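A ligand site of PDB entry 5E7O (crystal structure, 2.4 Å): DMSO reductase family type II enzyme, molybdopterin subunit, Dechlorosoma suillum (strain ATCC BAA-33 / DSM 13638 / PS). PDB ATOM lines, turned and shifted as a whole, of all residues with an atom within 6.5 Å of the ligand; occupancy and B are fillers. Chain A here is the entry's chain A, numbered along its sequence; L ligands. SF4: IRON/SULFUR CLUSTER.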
ATOM      1  N   ALA A  31       1.572 -15.351 -17.043  1.00  0.00           N
ATOM      2  CA  ALA A  31       0.141 -15.643 -17.077  1.00  0.00           C
ATOM      3  C   ALA A  31      -0.609 -14.494 -16.415  1.00  0.00           C
ATOM      4  O   ALA A  31      -0.052 -13.757 -15.607  1.00  0.00           O
ATOM      5  CB  ALA A  31      -0.182 -16.970 -16.381  1.00  0.00           C
ATOM      6  N   HIS A  32      -1.878 -14.354 -16.778  1.00  0.00           N
ATOM      7  CA  HIS A  32      -2.730 -13.312 -16.232  1.00  0.00           C
ATOM      8  C   HIS A  32      -3.661 -13.963 -15.200  1.00  0.00           C
ATOM      9  O   HIS A  32      -4.529 -14.764 -15.553  1.00  0.00           O
ATOM     10  CB  HIS A  32      -3.523 -12.620 -17.328  1.00  0.00           C
ATOM     11  CG  HIS A  32      -2.652 -12.055 -18.420  1.00  0.00           C
ATOM     12  ND1 HIS A  32      -2.295 -12.796 -19.536  1.00  0.00           N
ATOM     13  CD2 HIS A  32      -2.073 -10.849 -18.568  1.00  0.00           C
ATOM     14  CE1 HIS A  32      -1.533 -12.049 -20.315  1.00  0.00           C
ATOM     15  NE2 HIS A  32      -1.383 -10.864 -19.755  1.00  0.00           N
ATOM     16  N   LEU A  33      -3.469 -13.611 -13.936  1.00  0.00           N
ATOM     17  CA  LEU A  33      -4.124 -14.288 -12.824  1.00  0.00           C
ATOM     18  C   LEU A  33      -5.446 -13.593 -12.482  1.00  0.00           C
ATOM     19  O   LEU A  33      -5.631 -13.017 -11.411  1.00  0.00           O
ATOM     20  CB  LEU A  33      -3.196 -14.353 -11.620  1.00  0.00           C
ATOM     21  CG  LEU A  33      -1.760 -14.798 -11.946  1.00  0.00           C
ATOM     22  CD1 LEU A  33      -0.867 -14.693 -10.722  1.00  0.00           C
ATOM     23  CD2 LEU A  33      -1.755 -16.215 -12.500  1.00  0.00           C
ATOM     24  N   VAL A  34      -6.376 -13.664 -13.433  1.00  0.00           N
ATOM     25  CA  VAL A  34      -7.719 -13.132 -13.260  1.00  0.00           C
ATOM     26  C   VAL A  34      -8.722 -14.246 -13.537  1.00  0.00           C
ATOM     27  O   VAL A  34      -8.416 -15.256 -14.165  1.00  0.00           O
ATOM     28  CB  VAL A  34      -7.978 -11.914 -14.171  1.00  0.00           C
ATOM     29  CG1 VAL A  34      -7.181 -10.713 -13.686  1.00  0.00           C
ATOM     30  CG2 VAL A  34      -7.620 -12.233 -15.610  1.00  0.00           C
ATOM     31  N   ASN A  35      -9.943 -14.047 -13.033  1.00  0.00           N
ATOM     32  CA  ASN A  35     -11.007 -15.052 -13.158  1.00  0.00           C
ATOM     33  C   ASN A  35     -11.640 -14.906 -14.536  1.00  0.00           C
ATOM     34  O   ASN A  35     -12.706 -14.305 -14.724  1.00  0.00           O
ATOM     35  CB  ASN A  35     -12.037 -14.896 -12.049  1.00  0.00           C
ATOM     36  CG  ASN A  35     -13.099 -15.982 -12.083  1.00  0.00           C
ATOM     37  OD1 ASN A  35     -12.895 -17.042 -12.671  1.00  0.00           O
ATOM     38  ND2 ASN A  35     -14.236 -15.709 -11.457  1.00  0.00           N
ATOM     39  N   CYS A  36     -10.974 -15.513 -15.526  1.00  0.00           N
ATOM     40  CA  CYS A  36     -11.276 -15.306 -16.927  1.00  0.00           C
ATOM     41  C   CYS A  36     -11.529 -16.587 -17.700  1.00  0.00           C
ATOM     42  O   CYS A  36     -12.146 -16.519 -18.780  1.00  0.00           O
ATOM     43  CB  CYS A  36     -10.109 -14.576 -17.601  1.00  0.00           C
ATOM     44  SG  CYS A  36      -8.553 -15.370 -17.160  1.00  0.00           S
ATOM     45  N   THR A  37     -11.072 -17.732 -17.200  1.00  0.00           N
ATOM     46  CA  THR A  37     -11.073 -19.048 -17.847  1.00  0.00           C
ATOM     47  C   THR A  37     -10.109 -19.128 -19.016  1.00  0.00           C
ATOM     48  O   THR A  37     -10.042 -20.183 -19.676  1.00  0.00           O
ATOM     49  CB  THR A  37     -12.460 -19.475 -18.336  1.00  0.00           C
ATOM     50  OG1 THR A  37     -12.840 -18.671 -19.470  1.00  0.00           O
ATOM     51  CG2 THR A  37     -13.464 -19.298 -17.251  1.00  0.00           C
ATOM     52  N   GLY A  38      -9.354 -18.077 -19.315  1.00  0.00           N
ATOM     53  CA  GLY A  38      -8.404 -18.110 -20.407  1.00  0.00           C
ATOM     54  C   GLY A  38      -7.209 -18.984 -20.092  1.00  0.00           C
ATOM     55  O   GLY A  38      -6.969 -19.989 -20.777  1.00  0.00           O
ATOM     56  N   ALA A  39      -6.457 -18.613 -19.052  1.00  0.00           N
ATOM     57  CA  ALA A  39      -5.254 -19.336 -18.648  1.00  0.00           C
ATOM     58  C   ALA A  39      -4.307 -19.531 -19.837  1.00  0.00           C
ATOM     59  O   ALA A  39      -3.735 -20.603 -20.035  1.00  0.00           O
ATOM     60  CB  ALA A  39      -5.604 -20.671 -17.993  1.00  0.00           C
ATOM     61  N   CYS A  40      -4.153 -18.489 -20.620  1.00  0.00           N
ATOM     62  CA  CYS A  40      -3.441 -18.611 -21.879  1.00  0.00           C
ATOM     63  C   CYS A  40      -1.942 -18.434 -21.675  1.00  0.00           C
ATOM     64  O   CYS A  40      -1.512 -17.530 -20.954  1.00  0.00           O
ATOM     65  CB  CYS A  40      -3.948 -17.577 -22.880  1.00  0.00           C
ATOM     66  SG  CYS A  40      -5.711 -17.743 -23.223  1.00  0.00           S
ATOM     67  N   PRO A  41      -1.136 -19.297 -22.301  1.00  0.00           N
ATOM     68  CA  PRO A  41       0.317 -19.202 -22.142  1.00  0.00           C
ATOM     69  C   PRO A  41       0.862 -17.981 -22.868  1.00  0.00           C
ATOM     70  O   PRO A  41       0.562 -17.750 -24.045  1.00  0.00           O
ATOM     71  CB  PRO A  41       0.831 -20.509 -22.762  1.00  0.00           C
ATOM     72  CG  PRO A  41      -0.373 -21.405 -22.848  1.00  0.00           C
ATOM     73  CD  PRO A  41      -1.536 -20.495 -23.058  1.00  0.00           C
ATOM     74  N   HIS A  42       1.682 -17.199 -22.158  1.00  0.00           N
ATOM     75  CA  HIS A  42       2.255 -15.975 -22.693  1.00  0.00           C
ATOM     76  C   HIS A  42       3.760 -15.946 -22.468  1.00  0.00           C
ATOM     77  O   HIS A  42       4.296 -16.625 -21.594  1.00  0.00           O
ATOM     78  CB  HIS A  42       1.623 -14.721 -22.049  1.00  0.00           C
ATOM     79  CG  HIS A  42       0.294 -14.348 -22.628  1.00  0.00           C
ATOM     80  ND1 HIS A  42      -0.844 -15.081 -22.401  1.00  0.00           N
ATOM     81  CD2 HIS A  42      -0.072 -13.302 -23.398  1.00  0.00           C
ATOM     82  CE1 HIS A  42      -1.858 -14.510 -23.026  1.00  0.00           C
ATOM     83  NE2 HIS A  42      -1.418 -13.422 -23.634  1.00  0.00           N
ATOM     84  N   GLN A  56       1.182 -14.000 -26.737  1.00  0.00           N
ATOM     85  CA  GLN A  56       0.880 -15.425 -26.603  1.00  0.00           C
ATOM     86  C   GLN A  56       2.073 -16.260 -27.058  1.00  0.00           C
ATOM     87  O   GLN A  56       2.644 -16.015 -28.123  1.00  0.00           O
ATOM     88  CB  GLN A  56      -0.359 -15.776 -27.426  1.00  0.00           C
ATOM     89  CG  GLN A  56      -1.608 -14.962 -27.107  1.00  0.00           C
ATOM     90  CD  GLN A  56      -1.860 -13.877 -28.126  1.00  0.00           C
ATOM     91  OE1 GLN A  56      -1.004 -13.033 -28.398  1.00  0.00           O
ATOM     92  NE2 GLN A  56      -3.059 -13.883 -28.710  1.00  0.00           N
ATOM     93  N   ARG A  72      -4.660 -18.387 -28.568  1.00  0.00           N
ATOM     94  CA  ARG A  72      -5.355 -18.024 -27.350  1.00  0.00           C
ATOM     95  C   ARG A  72      -5.099 -16.548 -27.045  1.00  0.00           C
ATOM     96  O   ARG A  72      -4.675 -15.797 -27.937  1.00  0.00           O
ATOM     97  CB  ARG A  72      -4.942 -18.920 -26.177  1.00  0.00           C
ATOM     98  CG  ARG A  72      -5.506 -20.336 -26.213  1.00  0.00           C
ATOM     99  CD  ARG A  72      -5.449 -21.004 -24.843  1.00  0.00           C
ATOM    100  NE  ARG A  72      -6.500 -20.539 -23.941  1.00  0.00           N
ATOM    101  CZ  ARG A  72      -7.695 -21.120 -23.840  1.00  0.00           C
ATOM    102  NH1 ARG A  72      -7.990 -22.179 -24.566  1.00  0.00           N
ATOM    103  NH2 ARG A  72      -8.592 -20.630 -22.991  1.00  0.00           N
ATOM    104  N   GLY A  73      -5.362 -16.107 -25.813  1.00  0.00           N
ATOM    105  CA  GLY A  73      -5.195 -14.709 -25.462  1.00  0.00           C
ATOM    106  C   GLY A  73      -6.442 -13.886 -25.729  1.00  0.00           C
ATOM    107  O   GLY A  73      -7.467 -14.376 -26.211  1.00  0.00           O
ATOM    108  N   CYS A  74      -6.359 -12.602 -25.391  1.00  0.00           N
ATOM    109  CA  CYS A  74      -7.483 -11.698 -25.618  1.00  0.00           C
ATOM    110  C   CYS A  74      -6.971 -10.263 -25.624  1.00  0.00           C
ATOM    111  O   CYS A  74      -5.761 -10.009 -25.583  1.00  0.00           O
ATOM    112  CB  CYS A  74      -8.554 -11.876 -24.537  1.00  0.00           C
ATOM    113  SG  CYS A  74      -8.097 -11.102 -22.978  1.00  0.00           S
ATOM    114  N   ASN A  75      -7.904  -9.307 -25.688  1.00  0.00           N
ATOM    115  CA  ASN A  75      -7.575  -7.887 -25.716  1.00  0.00           C
ATOM    116  C   ASN A  75      -7.122  -7.369 -24.357  1.00  0.00           C
ATOM    117  O   ASN A  75      -6.317  -6.425 -24.291  1.00  0.00           O
ATOM    118  CB  ASN A  75      -8.779  -7.071 -26.191  1.00  0.00           C
ATOM    119  CG  ASN A  75     -10.063  -7.435 -25.453  1.00  0.00           C
ATOM    120  OD1 ASN A  75     -10.213  -8.557 -24.951  1.00  0.00           O
ATOM    121  ND2 ASN A  75     -10.990  -6.493 -25.376  1.00  0.00           N
ATOM    122  N   LYS A  76      -7.624  -7.948 -23.269  1.00  0.00           N
ATOM    123  CA  LYS A  76      -7.162  -7.543 -21.943  1.00  0.00           C
ATOM    124  C   LYS A  76      -5.778  -8.101 -21.642  1.00  0.00           C
ATOM    125  O   LYS A  76      -4.932  -7.401 -21.056  1.00  0.00           O
ATOM    126  CB  LYS A  76      -8.155  -7.994 -20.860  1.00  0.00           C
ATOM    127  CG  LYS A  76      -9.472  -7.231 -20.839  1.00  0.00           C
ATOM    128  CD  LYS A  76     -10.462  -7.753 -21.861  1.00  0.00           C
ATOM    129  CE  LYS A  76     -10.953  -9.149 -21.509  1.00  0.00           C
ATOM    130  NZ  LYS A  76     -11.559  -9.831 -22.690  1.00  0.00           N
ATOM    131  N   GLY A  77      -5.508  -9.347 -22.056  1.00  0.00           N
ATOM    132  CA  GLY A  77      -4.229  -9.950 -21.770  1.00  0.00           C
ATOM    133  C   GLY A  77      -3.075  -9.323 -22.538  1.00  0.00           C
ATOM    134  O   GLY A  77      -1.943  -9.305 -22.043  1.00  0.00           O
ATOM    135  N   GLU A  78      -3.338  -8.816 -23.740  1.00  0.00           N
ATOM    136  CA  GLU A  78      -2.285  -8.217 -24.544  1.00  0.00           C
ATOM    137  C   GLU A  78      -1.918  -6.803 -24.099  1.00  0.00           C
ATOM    138  O   GLU A  78      -1.043  -6.186 -24.713  1.00  0.00           O
ATOM    139  CB  GLU A  78      -2.689  -8.204 -26.023  1.00  0.00           C
ATOM    140  CG  GLU A  78      -2.632  -9.565 -26.689  1.00  0.00           C
ATOM    141  CD  GLU A  78      -1.522 -10.445 -26.128  1.00  0.00           C
ATOM    142  OE1 GLU A  78      -1.839 -11.513 -25.572  1.00  0.00           O
ATOM    143  OE2 GLU A  78      -0.337 -10.058 -26.232  1.00  0.00           O
ATOM    144  N   ILE A 209     -13.405 -15.747 -25.314  1.00  0.00           N
ATOM    145  CA  ILE A 209     -12.657 -15.243 -26.457  1.00  0.00           C
ATOM    146  C   ILE A 209     -11.530 -16.186 -26.887  1.00  0.00           C
ATOM    147  O   ILE A 209     -11.440 -16.485 -28.094  1.00  0.00           O
ATOM    148  CB  ILE A 209     -12.148 -13.818 -26.175  1.00  0.00           C
ATOM    149  CG1 ILE A 209     -13.334 -12.844 -26.141  1.00  0.00           C
ATOM    150  CG2 ILE A 209     -11.118 -13.387 -27.201  1.00  0.00           C
ATOM    151  CD1 ILE A 209     -12.940 -11.415 -25.869  1.00  0.00           C
ATOM    152  N   PRO A 210     -10.664 -16.688 -25.999  1.00  0.00           N
ATOM    153  CA  PRO A 210      -9.597 -17.582 -26.465  1.00  0.00           C
ATOM    154  C   PRO A 210     -10.094 -18.928 -26.971  1.00  0.00           C
ATOM    155  O   PRO A 210      -9.326 -19.630 -27.653  1.00  0.00           O
ATOM    156  CB  PRO A 210      -8.698 -17.748 -25.223  1.00  0.00           C
ATOM    157  CG  PRO A 210      -9.612 -17.503 -24.088  1.00  0.00           C
ATOM    158  CD  PRO A 210     -10.553 -16.438 -24.546  1.00  0.00           C
ATOM    159  N   GLN A 460     -13.283 -19.518 -13.827  1.00  0.00           N
ATOM    160  CA  GLN A 460     -12.118 -20.405 -13.874  1.00  0.00           C
ATOM    161  C   GLN A 460     -12.136 -21.310 -12.634  1.00  0.00           C
ATOM    162  O   GLN A 460     -11.347 -21.179 -11.705  1.00  0.00           O
ATOM    163  CB  GLN A 460     -10.856 -19.569 -13.955  1.00  0.00           C
ATOM    164  CG  GLN A 460      -9.635 -20.268 -14.494  1.00  0.00           C
ATOM    165  CD  GLN A 460      -8.569 -19.284 -14.942  1.00  0.00           C
ATOM    166  OE1 GLN A 460      -8.882 -18.228 -15.502  1.00  0.00           O
ATOM    167  NE2 GLN A 460      -7.314 -19.610 -14.691  1.00  0.00           N
ATOM    168  N   ASN A 591      -1.541 -21.603 -12.787  1.00  0.00           N
ATOM    169  CA  ASN A 591      -2.712 -21.023 -13.427  1.00  0.00           C
ATOM    170  C   ASN A 591      -3.356 -22.020 -14.380  1.00  0.00           C
ATOM    171  O   ASN A 591      -2.784 -22.340 -15.422  1.00  0.00           O
ATOM    172  CB  ASN A 591      -2.317 -19.731 -14.159  1.00  0.00           C
ATOM    173  CG  ASN A 591      -3.479 -19.088 -14.885  1.00  0.00           C
ATOM    174  OD1 ASN A 591      -3.470 -18.984 -16.113  1.00  0.00           O
ATOM    175  ND2 ASN A 591      -4.490 -18.664 -14.137  1.00  0.00           N
ATOM    176  N   ASN A 600      -0.807 -23.873 -16.915  1.00  0.00           N
ATOM    177  CA  ASN A 600      -0.105 -22.636 -17.212  1.00  0.00           C
ATOM    178  C   ASN A 600       0.448 -22.042 -15.928  1.00  0.00           C
ATOM    179  O   ASN A 600       0.081 -22.439 -14.823  1.00  0.00           O
ATOM    180  CB  ASN A 600      -1.041 -21.648 -17.920  1.00  0.00           C
ATOM    181  CG  ASN A 600      -0.296 -20.504 -18.569  1.00  0.00           C
ATOM    182  OD1 ASN A 600       0.841 -20.656 -19.010  1.00  0.00           O
ATOM    183  ND2 ASN A 600      -0.941 -19.338 -18.637  1.00  0.00           N
ATOM    184  N   VAL A 769     -12.132  -8.244 -17.750  1.00  0.00           N
ATOM    185  CA  VAL A 769     -12.317  -9.464 -16.978  1.00  0.00           C
ATOM    186  C   VAL A 769     -12.856  -9.045 -15.621  1.00  0.00           C
ATOM    187  O   VAL A 769     -12.098  -8.707 -14.706  1.00  0.00           O
ATOM    188  CB  VAL A 769     -11.011 -10.261 -16.830  1.00  0.00           C
ATOM    189  CG1 VAL A 769     -11.223 -11.483 -15.950  1.00  0.00           C
ATOM    190  CG2 VAL A 769     -10.488 -10.684 -18.202  1.00  0.00           C
ATOM    191  N   PHE A 773      -9.493  -4.526 -15.594  1.00  0.00           N
ATOM    192  CA  PHE A 773      -9.449  -3.911 -16.924  1.00  0.00           C
ATOM    193  C   PHE A 773     -10.655  -3.012 -17.192  1.00  0.00           C
ATOM    194  O   PHE A 773     -10.747  -2.452 -18.292  1.00  0.00           O
ATOM    195  CB  PHE A 773      -9.327  -4.938 -18.056  1.00  0.00           C
ATOM    196  CG  PHE A 773      -8.077  -5.761 -17.980  1.00  0.00           C
ATOM    197  CD1 PHE A 773      -6.884  -5.273 -18.491  1.00  0.00           C
ATOM    198  CD2 PHE A 773      -8.094  -7.022 -17.421  1.00  0.00           C
ATOM    199  CE1 PHE A 773      -5.729  -6.028 -18.422  1.00  0.00           C
ATOM    200  CE2 PHE A 773      -6.948  -7.787 -17.354  1.00  0.00           C
ATOM    201  CZ  PHE A 773      -5.758  -7.290 -17.857  1.00  0.00           C
HETATM  202 FE1  SF4 L   1      -7.042 -12.764 -22.071  1.00  0.00          FE
HETATM  203 FE2  SF4 L   1      -7.754 -14.266 -19.492  1.00  0.00          FE
HETATM  204 FE3  SF4 L   1      -4.911 -13.185 -19.877  1.00  0.00          FE
HETATM  205 FE4  SF4 L   1      -5.884 -15.576 -21.517  1.00  0.00          FE
HETATM  206  S1  SF4 L   1      -5.754 -15.139 -19.386  1.00  0.00           S
HETATM  207  S2  SF4 L   1      -5.038 -13.622 -22.017  1.00  0.00           S
HETATM  208  S3  SF4 L   1      -7.899 -14.725 -21.627  1.00  0.00           S
HETATM  209  S4  SF4 L   1      -6.911 -12.296 -19.930  1.00  0.00           S
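Residues that only touch the ligand: Gly 38 (3.6 Å), His 42 (3.5 Å), Gly 73 (3.6 Å) and Gly 77 (3.7 Å).
Hydrophobic or aromatic side chains that line the ligand: His 32 and His 42.
Of the 27 residues printed, 9 come within 4 Å of the ligand.
N of Lys 76 lies close to SG of Cys 74, at 3.2 Å.
NE2 of His 32 lies within hydrogen-bond range of O of Gly 77 (2.8 Å).
The side-chain sulfur (SG) of Cys 36 lies close to the backbone NH (N) of Gly 38, 3.6 Å away.
A ring nitrogen (ND1) of His 42 is in hydrogen-bond range of the backbone carbonyl oxygen (O) of Cys 40, 2.9 Å away.
SG of Cys 40 lies close to NE of Arg 72 (3.0 Å).
A ring nitrogen (NE2) of His 42 sits at hydrogen-bond distance from the side-chain carboxylate (OE1) of Glu 78, 2.8 Å away.
The backbone carbonyl oxygen (O) of Ala 39 lies within hydrogen-bond range of the side-chain amide nitrogen (ND2) of Asn 600 (3.4 Å).
O of Gly 38 sits at hydrogen-bond distance from NH2 of Arg 72 (2.8 Å).
A sulfur (S2) of the ligand sits close to the backbone NH (N) of Cys 74, 3.8 Å away.
The side-chain sulfur (SG) of Cys 74 binds an iron atom (FE1) of the ligand.
A ring nitrogen (ND1) of His 32 lies close to a sulfur (S2) of the ligand.
The side-chain sulfur (SG) of Cys 36 is bound to an iron atom (FE2) of the ligand, 2.7 Å away.
The side-chain sulfur (SG) of Cys 40 is bound to an iron atom (FE4) of the ligand (2.8 Å).
N of Ala 39 lies close to S1 of the ligand, 3.6 Å away.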
